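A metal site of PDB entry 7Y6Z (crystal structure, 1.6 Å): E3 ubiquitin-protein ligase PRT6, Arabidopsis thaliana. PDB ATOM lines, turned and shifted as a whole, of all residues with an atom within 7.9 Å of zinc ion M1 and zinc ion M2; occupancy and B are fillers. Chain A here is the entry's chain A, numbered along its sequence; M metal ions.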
ATOM      1  N   GLY A   7     -16.359  13.693 -29.004  1.00  0.00           N
ATOM      2  CA  GLY A   7     -15.164  14.126 -29.747  1.00  0.00           C
ATOM      3  C   GLY A   7     -14.323  14.952 -28.766  1.00  0.00           C
ATOM      4  O   GLY A   7     -14.775  15.089 -27.641  1.00  0.00           O
ATOM      5  N   VAL A   8     -13.149  15.472 -29.174  1.00  0.00           N
ATOM      6  CA  VAL A   8     -12.335  16.398 -28.371  1.00  0.00           C
ATOM      7  C   VAL A   8     -12.133  17.703 -29.142  1.00  0.00           C
ATOM      8  O   VAL A   8     -11.606  17.683 -30.267  1.00  0.00           O
ATOM      9  CB  VAL A   8     -10.972  15.793 -28.045  1.00  0.00           C
ATOM     10  CG1 VAL A   8     -10.399  15.238 -29.379  1.00  0.00           C
ATOM     11  CG2 VAL A   8     -10.083  16.887 -27.444  1.00  0.00           C
ATOM     12  N   CYS A   9     -12.454  18.845 -28.518  1.00  0.00           N
ATOM     13  CA  CYS A   9     -12.439  20.093 -29.269  1.00  0.00           C
ATOM     14  C   CYS A   9     -11.026  20.475 -29.683  1.00  0.00           C
ATOM     15  O   CYS A   9     -10.106  20.563 -28.887  1.00  0.00           O
ATOM     16  CB  CYS A   9     -13.042  21.276 -28.474  1.00  0.00           C
ATOM     17  SG  CYS A   9     -13.014  22.835 -29.487  1.00  0.00           S
ATOM     18  N   GLY A  10     -10.866  20.795 -30.950  1.00  0.00           N
ATOM     19  CA  GLY A  10      -9.553  21.237 -31.331  1.00  0.00           C
ATOM     20  C   GLY A  10      -9.148  22.570 -30.723  1.00  0.00           C
ATOM     21  O   GLY A  10      -8.148  22.681 -30.003  1.00  0.00           O
ATOM     22  N   SER A  11      -9.946  23.570 -31.066  1.00  0.00           N
ATOM     23  CA  SER A  11      -9.624  24.976 -30.986  1.00  0.00           C
ATOM     24  C   SER A  11      -8.465  25.480 -30.157  1.00  0.00           C
ATOM     25  O   SER A  11      -8.385  25.327 -28.928  1.00  0.00           O
ATOM     26  CB  SER A  11     -10.884  25.727 -30.567  1.00  0.00           C
ATOM     27  OG  SER A  11     -11.986  25.291 -31.327  1.00  0.00           O
ATOM     28  N   VAL A  12      -7.616  26.194 -30.893  1.00  0.00           N
ATOM     29  CA  VAL A  12      -6.409  26.840 -30.411  1.00  0.00           C
ATOM     30  C   VAL A  12      -6.648  28.317 -30.344  1.00  0.00           C
ATOM     31  O   VAL A  12      -7.215  28.894 -31.295  1.00  0.00           O
ATOM     32  CB  VAL A  12      -5.237  26.502 -31.353  1.00  0.00           C
ATOM     33  CG1 VAL A  12      -3.965  27.226 -30.960  1.00  0.00           C
ATOM     34  CG2 VAL A  12      -5.047  25.017 -31.334  1.00  0.00           C
ATOM     35  N   TRP A  13      -6.207  28.957 -29.247  1.00  0.00           N
ATOM     36  CA  TRP A  13      -6.264  30.398 -29.039  1.00  0.00           C
ATOM     37  C   TRP A  13      -4.903  30.987 -29.317  1.00  0.00           C
ATOM     38  O   TRP A  13      -3.888  30.386 -29.024  1.00  0.00           O
ATOM     39  CB  TRP A  13      -6.663  30.766 -27.593  1.00  0.00           C
ATOM     40  CG  TRP A  13      -7.876  30.116 -27.218  1.00  0.00           C
ATOM     41  CD1 TRP A  13      -9.045  30.240 -27.839  1.00  0.00           C
ATOM     42  CD2 TRP A  13      -8.059  29.144 -26.190  1.00  0.00           C
ATOM     43  NE1 TRP A  13      -9.974  29.432 -27.274  1.00  0.00           N
ATOM     44  CE2 TRP A  13      -9.413  28.758 -26.248  1.00  0.00           C
ATOM     45  CE3 TRP A  13      -7.245  28.602 -25.194  1.00  0.00           C
ATOM     46  CZ2 TRP A  13      -9.971  27.850 -25.358  1.00  0.00           C
ATOM     47  CZ3 TRP A  13      -7.788  27.658 -24.355  1.00  0.00           C
ATOM     48  CH2 TRP A  13      -9.138  27.292 -24.450  1.00  0.00           C
ATOM     49  N   ALA A  32      -9.627  25.469 -19.648  1.00  0.00           N
ATOM     50  CA  ALA A  32     -10.471  26.509 -20.250  1.00  0.00           C
ATOM     51  C   ALA A  32     -11.219  25.923 -21.438  1.00  0.00           C
ATOM     52  O   ALA A  32     -10.786  24.922 -22.003  1.00  0.00           O
ATOM     53  CB  ALA A  32      -9.675  27.730 -20.761  1.00  0.00           C
ATOM     54  N   ILE A  33     -12.337  26.552 -21.811  1.00  0.00           N
ATOM     55  CA  ILE A  33     -13.004  26.082 -23.027  1.00  0.00           C
ATOM     56  C   ILE A  33     -13.299  27.254 -23.935  1.00  0.00           C
ATOM     57  O   ILE A  33     -13.537  28.375 -23.457  1.00  0.00           O
ATOM     58  CB  ILE A  33     -14.270  25.263 -22.804  1.00  0.00           C
ATOM     59  CG1 ILE A  33     -15.309  26.028 -22.008  1.00  0.00           C
ATOM     60  CG2 ILE A  33     -13.838  23.966 -22.038  1.00  0.00           C
ATOM     61  CD1 ILE A  33     -16.621  25.272 -21.951  1.00  0.00           C
ATOM     62  N   CYS A  34     -13.307  26.977 -25.223  1.00  0.00           N
ATOM     63  CA  CYS A  34     -13.563  28.042 -26.182  1.00  0.00           C
ATOM     64  C   CYS A  34     -14.980  28.544 -26.041  1.00  0.00           C
ATOM     65  O   CYS A  34     -15.874  27.849 -25.557  1.00  0.00           O
ATOM     66  CB  CYS A  34     -13.279  27.534 -27.630  1.00  0.00           C
ATOM     67  SG  CYS A  34     -14.382  26.356 -28.343  1.00  0.00           S
ATOM     68  N   VAL A  35     -15.238  29.742 -26.583  1.00  0.00           N
ATOM     69  CA  VAL A  35     -16.548  30.355 -26.439  1.00  0.00           C
ATOM     70  C   VAL A  35     -17.622  29.486 -27.059  1.00  0.00           C
ATOM     71  O   VAL A  35     -18.703  29.331 -26.433  1.00  0.00           O
ATOM     72  CB  VAL A  35     -16.551  31.769 -27.043  1.00  0.00           C
ATOM     73  CG1 VAL A  35     -17.980  32.344 -27.039  1.00  0.00           C
ATOM     74  CG2 VAL A  35     -15.596  32.602 -26.270  1.00  0.00           C
ATOM     75  N   PRO A  36     -17.491  28.969 -28.293  1.00  0.00           N
ATOM     76  CA  PRO A  36     -18.559  28.137 -28.852  1.00  0.00           C
ATOM     77  C   PRO A  36     -18.883  26.913 -27.982  1.00  0.00           C
ATOM     78  O   PRO A  36     -20.057  26.585 -27.809  1.00  0.00           O
ATOM     79  CB  PRO A  36     -18.028  27.735 -30.228  1.00  0.00           C
ATOM     80  CG  PRO A  36     -16.825  28.544 -30.479  1.00  0.00           C
ATOM     81  CD  PRO A  36     -16.350  29.126 -29.220  1.00  0.00           C
ATOM     82  N   CYS A  37     -17.874  26.233 -27.457  1.00  0.00           N
ATOM     83  CA  CYS A  37     -18.180  25.103 -26.571  1.00  0.00           C
ATOM     84  C   CYS A  37     -18.878  25.579 -25.289  1.00  0.00           C
ATOM     85  O   CYS A  37     -19.776  24.892 -24.755  1.00  0.00           O
ATOM     86  CB  CYS A  37     -16.911  24.294 -26.269  1.00  0.00           C
ATOM     87  SG  CYS A  37     -16.110  23.432 -27.586  1.00  0.00           S
ATOM     88  N   PHE A  38     -18.437  26.693 -24.715  1.00  0.00           N
ATOM     89  CA  PHE A  38     -19.162  27.229 -23.539  1.00  0.00           C
ATOM     90  C   PHE A  38     -20.609  27.462 -23.855  1.00  0.00           C
ATOM     91  O   PHE A  38     -21.511  27.171 -23.070  1.00  0.00           O
ATOM     92  CB  PHE A  38     -18.553  28.554 -23.072  1.00  0.00           C
ATOM     93  CG  PHE A  38     -19.257  29.155 -21.865  1.00  0.00           C
ATOM     94  CD1 PHE A  38     -18.943  28.704 -20.571  1.00  0.00           C
ATOM     95  CD2 PHE A  38     -20.231  30.145 -22.020  1.00  0.00           C
ATOM     96  CE1 PHE A  38     -19.536  29.258 -19.456  1.00  0.00           C
ATOM     97  CE2 PHE A  38     -20.851  30.685 -20.887  1.00  0.00           C
ATOM     98  CZ  PHE A  38     -20.489  30.221 -19.613  1.00  0.00           C
ATOM     99  N   ASN A  40     -22.459  26.090 -26.148  1.00  0.00           N
ATOM    100  CA  ASN A  40     -23.248  24.924 -26.475  1.00  0.00           C
ATOM    101  C   ASN A  40     -23.291  23.906 -25.321  1.00  0.00           C
ATOM    102  O   ASN A  40     -23.694  22.776 -25.543  1.00  0.00           O
ATOM    103  CB  ASN A  40     -22.743  24.254 -27.753  1.00  0.00           C
ATOM    104  CG  ASN A  40     -23.013  25.071 -28.973  1.00  0.00           C
ATOM    105  OD1 ASN A  40     -24.006  25.750 -29.072  1.00  0.00           O
ATOM    106  ND2 ASN A  40     -22.118  24.995 -29.937  1.00  0.00           N
ATOM    107  N   GLY A  41     -22.927  24.326 -24.113  1.00  0.00           N
ATOM    108  CA  GLY A  41     -23.067  23.516 -22.939  1.00  0.00           C
ATOM    109  C   GLY A  41     -23.932  24.211 -21.921  1.00  0.00           C
ATOM    110  O   GLY A  41     -24.553  25.220 -22.230  1.00  0.00           O
ATOM    111  N   CYS A  57      -5.420  25.730 -25.721  1.00  0.00           N
ATOM    112  CA  CYS A  57      -6.369  24.939 -26.511  1.00  0.00           C
ATOM    113  C   CYS A  57      -7.570  24.551 -25.654  1.00  0.00           C
ATOM    114  O   CYS A  57      -7.483  24.412 -24.441  1.00  0.00           O
ATOM    115  CB  CYS A  57      -5.688  23.680 -27.129  1.00  0.00           C
ATOM    116  SG  CYS A  57      -5.062  22.438 -26.027  1.00  0.00           S
ATOM    117  N   CYS A  58      -8.722  24.406 -26.311  1.00  0.00           N
ATOM    118  CA  CYS A  58      -9.966  24.111 -25.594  1.00  0.00           C
ATOM    119  C   CYS A  58      -9.929  22.691 -25.030  1.00  0.00           C
ATOM    120  O   CYS A  58      -9.504  21.750 -25.717  1.00  0.00           O
ATOM    121  CB  CYS A  58     -11.171  24.281 -26.540  1.00  0.00           C
ATOM    122  SG  CYS A  58     -12.777  23.876 -25.850  1.00  0.00           S
ATOM    123  N   ASP A  59     -10.425  22.545 -23.803  1.00  0.00           N
ATOM    124  CA  ASP A  59     -10.422  21.255 -23.081  1.00  0.00           C
ATOM    125  C   ASP A  59     -11.755  20.530 -23.173  1.00  0.00           C
ATOM    126  O   ASP A  59     -11.907  19.447 -22.630  1.00  0.00           O
ATOM    127  CB  ASP A  59     -10.075  21.476 -21.614  1.00  0.00           C
ATOM    128  CG  ASP A  59      -8.678  21.981 -21.424  1.00  0.00           C
ATOM    129  OD1 ASP A  59      -7.738  21.340 -21.932  1.00  0.00           O
ATOM    130  OD2 ASP A  59      -8.486  23.002 -20.699  1.00  0.00           O
ATOM    131  N   CYS A  60     -12.722  21.072 -23.878  1.00  0.00           N
ATOM    132  CA  CYS A  60     -14.028  20.467 -24.027  1.00  0.00           C
ATOM    133  C   CYS A  60     -13.885  19.150 -24.757  1.00  0.00           C
ATOM    134  O   CYS A  60     -13.279  19.086 -25.841  1.00  0.00           O
ATOM    135  CB  CYS A  60     -14.998  21.355 -24.793  1.00  0.00           C
ATOM    136  SG  CYS A  60     -16.615  20.791 -24.917  1.00  0.00           S
ATOM    137  N   GLY A  61     -14.421  18.101 -24.130  1.00  0.00           N
ATOM    138  CA  GLY A  61     -14.329  16.767 -24.645  1.00  0.00           C
ATOM    139  C   GLY A  61     -13.232  15.951 -24.041  1.00  0.00           C
ATOM    140  O   GLY A  61     -13.234  14.735 -24.235  1.00  0.00           O
ATOM    141  N   ASP A  62     -12.287  16.591 -23.325  1.00  0.00           N
ATOM    142  CA  ASP A  62     -11.187  15.905 -22.654  1.00  0.00           C
ATOM    143  C   ASP A  62     -11.559  15.722 -21.193  1.00  0.00           C
ATOM    144  O   ASP A  62     -11.467  16.669 -20.410  1.00  0.00           O
ATOM    145  CB  ASP A  62      -9.905  16.726 -22.837  1.00  0.00           C
ATOM    146  CG  ASP A  62      -8.674  16.095 -22.221  1.00  0.00           C
ATOM    147  OD1 ASP A  62      -8.757  14.988 -21.630  1.00  0.00           O
ATOM    148  OD2 ASP A  62      -7.589  16.726 -22.286  1.00  0.00           O
ATOM    149  N   TRP A  66     -11.487  18.419 -18.083  1.00  0.00           N
ATOM    150  CA  TRP A  66     -12.775  19.062 -17.914  1.00  0.00           C
ATOM    151  C   TRP A  66     -13.774  18.013 -17.497  1.00  0.00           C
ATOM    152  O   TRP A  66     -13.773  16.893 -18.015  1.00  0.00           O
ATOM    153  CB  TRP A  66     -13.154  19.715 -19.242  1.00  0.00           C
ATOM    154  CG  TRP A  66     -14.168  20.807 -19.210  1.00  0.00           C
ATOM    155  CD1 TRP A  66     -15.486  20.692 -19.518  1.00  0.00           C
ATOM    156  CD2 TRP A  66     -13.943  22.215 -18.874  1.00  0.00           C
ATOM    157  NE1 TRP A  66     -16.106  21.913 -19.364  1.00  0.00           N
ATOM    158  CE2 TRP A  66     -15.180  22.867 -18.997  1.00  0.00           C
ATOM    159  CE3 TRP A  66     -12.821  22.952 -18.541  1.00  0.00           C
ATOM    160  CZ2 TRP A  66     -15.321  24.246 -18.834  1.00  0.00           C
ATOM    161  CZ3 TRP A  66     -12.927  24.271 -18.287  1.00  0.00           C
ATOM    162  CH2 TRP A  66     -14.197  24.928 -18.427  1.00  0.00           C
ATOM    163  N   GLY A  70     -19.708  19.254 -18.041  1.00  0.00           N
ATOM    164  CA  GLY A  70     -19.438  20.517 -18.698  1.00  0.00           C
ATOM    165  C   GLY A  70     -19.085  20.465 -20.155  1.00  0.00           C
ATOM    166  O   GLY A  70     -18.860  21.542 -20.757  1.00  0.00           O
ATOM    167  N   PHE A  71     -19.116  19.292 -20.775  1.00  0.00           N
ATOM    168  CA  PHE A  71     -18.928  19.154 -22.215  1.00  0.00           C
ATOM    169  C   PHE A  71     -20.107  19.785 -22.966  1.00  0.00           C
ATOM    170  O   PHE A  71     -21.244  19.835 -22.468  1.00  0.00           O
ATOM    171  CB  PHE A  71     -18.846  17.688 -22.618  1.00  0.00           C
ATOM    172  CG  PHE A  71     -17.642  16.954 -22.095  1.00  0.00           C
ATOM    173  CD1 PHE A  71     -17.521  15.603 -22.243  1.00  0.00           C
ATOM    174  CD2 PHE A  71     -16.610  17.651 -21.463  1.00  0.00           C
ATOM    175  CE1 PHE A  71     -16.393  14.942 -21.734  1.00  0.00           C
ATOM    176  CE2 PHE A  71     -15.482  17.058 -21.085  1.00  0.00           C
ATOM    177  CZ  PHE A  71     -15.356  15.680 -21.204  1.00  0.00           C
ATOM    178  N   CYS A  72     -19.793  20.312 -24.146  1.00  0.00           N
ATOM    179  CA  CYS A  72     -20.796  20.812 -25.066  1.00  0.00           C
ATOM    180  C   CYS A  72     -21.495  19.680 -25.834  1.00  0.00           C
ATOM    181  O   CYS A  72     -21.138  18.503 -25.748  1.00  0.00           O
ATOM    182  CB  CYS A  72     -20.225  21.882 -26.027  1.00  0.00           C
ATOM    183  SG  CYS A  72     -19.372  21.383 -27.371  1.00  0.00           S
ATOM    184  N   SER A  73     -22.542  20.090 -26.580  1.00  0.00           N
ATOM    185  CA  SER A  73     -23.342  19.268 -27.481  1.00  0.00           C
ATOM    186  C   SER A  73     -22.517  18.445 -28.461  1.00  0.00           C
ATOM    187  O   SER A  73     -22.881  17.300 -28.773  1.00  0.00           O
ATOM    188  CB  SER A  73     -24.297  20.184 -28.279  1.00  0.00           C
ATOM    189  OG  SER A  73     -23.776  20.471 -29.571  1.00  0.00           O
ATOM    190  N   ASN A  74     -21.405  18.988 -28.948  1.00  0.00           N
ATOM    191  CA  ASN A  74     -20.653  18.364 -30.032  1.00  0.00           C
ATOM    192  C   ASN A  74     -19.464  17.549 -29.568  1.00  0.00           C
ATOM    193  O   ASN A  74     -18.801  16.913 -30.412  1.00  0.00           O
ATOM    194  CB  ASN A  74     -20.157  19.422 -31.033  1.00  0.00           C
ATOM    195  CG  ASN A  74     -21.272  20.354 -31.510  1.00  0.00           C
ATOM    196  OD1 ASN A  74     -22.309  19.914 -32.007  1.00  0.00           O
ATOM    197  ND2 ASN A  74     -21.047  21.665 -31.349  1.00  0.00           N
ATOM    198  N   HIS A  75     -19.193  17.472 -28.245  1.00  0.00           N
ATOM    199  CA  HIS A  75     -17.973  16.807 -27.799  1.00  0.00           C
ATOM    200  C   HIS A  75     -18.255  15.716 -26.796  1.00  0.00           C
ATOM    201  O   HIS A  75     -17.441  15.447 -25.931  1.00  0.00           O
ATOM    202  CB  HIS A  75     -16.940  17.820 -27.284  1.00  0.00           C
ATOM    203  CG  HIS A  75     -16.482  18.753 -28.383  1.00  0.00           C
ATOM    204  ND1 HIS A  75     -16.844  20.086 -28.460  1.00  0.00           N
ATOM    205  CD2 HIS A  75     -15.784  18.500 -29.523  1.00  0.00           C
ATOM    206  CE1 HIS A  75     -16.336  20.619 -29.544  1.00  0.00           C
ATOM    207  NE2 HIS A  75     -15.719  19.666 -30.235  1.00  0.00           N
ATOM    208  N   LYS A  76     -19.405  15.048 -26.935  1.00  0.00           N
ATOM    209  CA  LYS A  76     -19.760  13.973 -26.017  1.00  0.00           C
ATOM    210  C   LYS A  76     -19.824  12.625 -26.726  1.00  0.00           C
ATOM    211  O   LYS A  76     -19.777  11.563 -26.046  1.00  0.00           O
ATOM    212  CB  LYS A  76     -21.089  14.274 -25.359  1.00  0.00           C
ATOM    213  CG  LYS A  76     -21.097  15.478 -24.565  1.00  0.00           C
ATOM    214  CD  LYS A  76     -22.544  15.840 -24.315  1.00  0.00           C
ATOM    215  CE  LYS A  76     -22.728  16.805 -23.175  1.00  0.00           C
ATOM    216  NZ  LYS A  76     -24.186  16.958 -22.773  1.00  0.00           N
HETATM  217 ZN    ZN M   1     -17.166  21.309 -26.982  1.00  0.00          ZN
HETATM  218 ZN    ZN M   2     -14.014  24.124 -27.772  1.00  0.00          ZN
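Zinc ion M2 is bound by the side-chain sulfur (SG) of Cys 37, the side-chain sulfur (SG) of Cys 58, the side-chain sulfur (SG) of Cys 34 and the side-chain sulfur (SG) of Cys 9.
Within 4 Å of zinc ion M2: Cys 9, Cys 34, Cys 37 and Cys 58. The nearest printed residue that does not touch zinc ion M2 is Cys 60 (4.2 Å).
N of Cys 58 sits at hydrogen-bond distance from O of Ser 11 (2.8 Å). The backbone NH (N) of Cys 60 sits close to the side-chain sulfur (SG) of Cys 58. The backbone carbonyl oxygen (O) of Cys 60 sits at hydrogen-bond distance from the backbone NH (N) of Cys 9. The side-chain hydroxyl of Ser 11 lies close to the side-chain sulfur of Cys 9, 3.2 Å away. The side-chain sulfur (SG) of Cys 72 sits close to the backbone NH (N) of Asn 74 (3.5 Å).
Zinc ion M1 is bound by ND1 of His 75, SG of Cys 60, SG of Cys 72 and SG of Cys 37. Zinc ion M1 has four donor atoms within binding distance.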
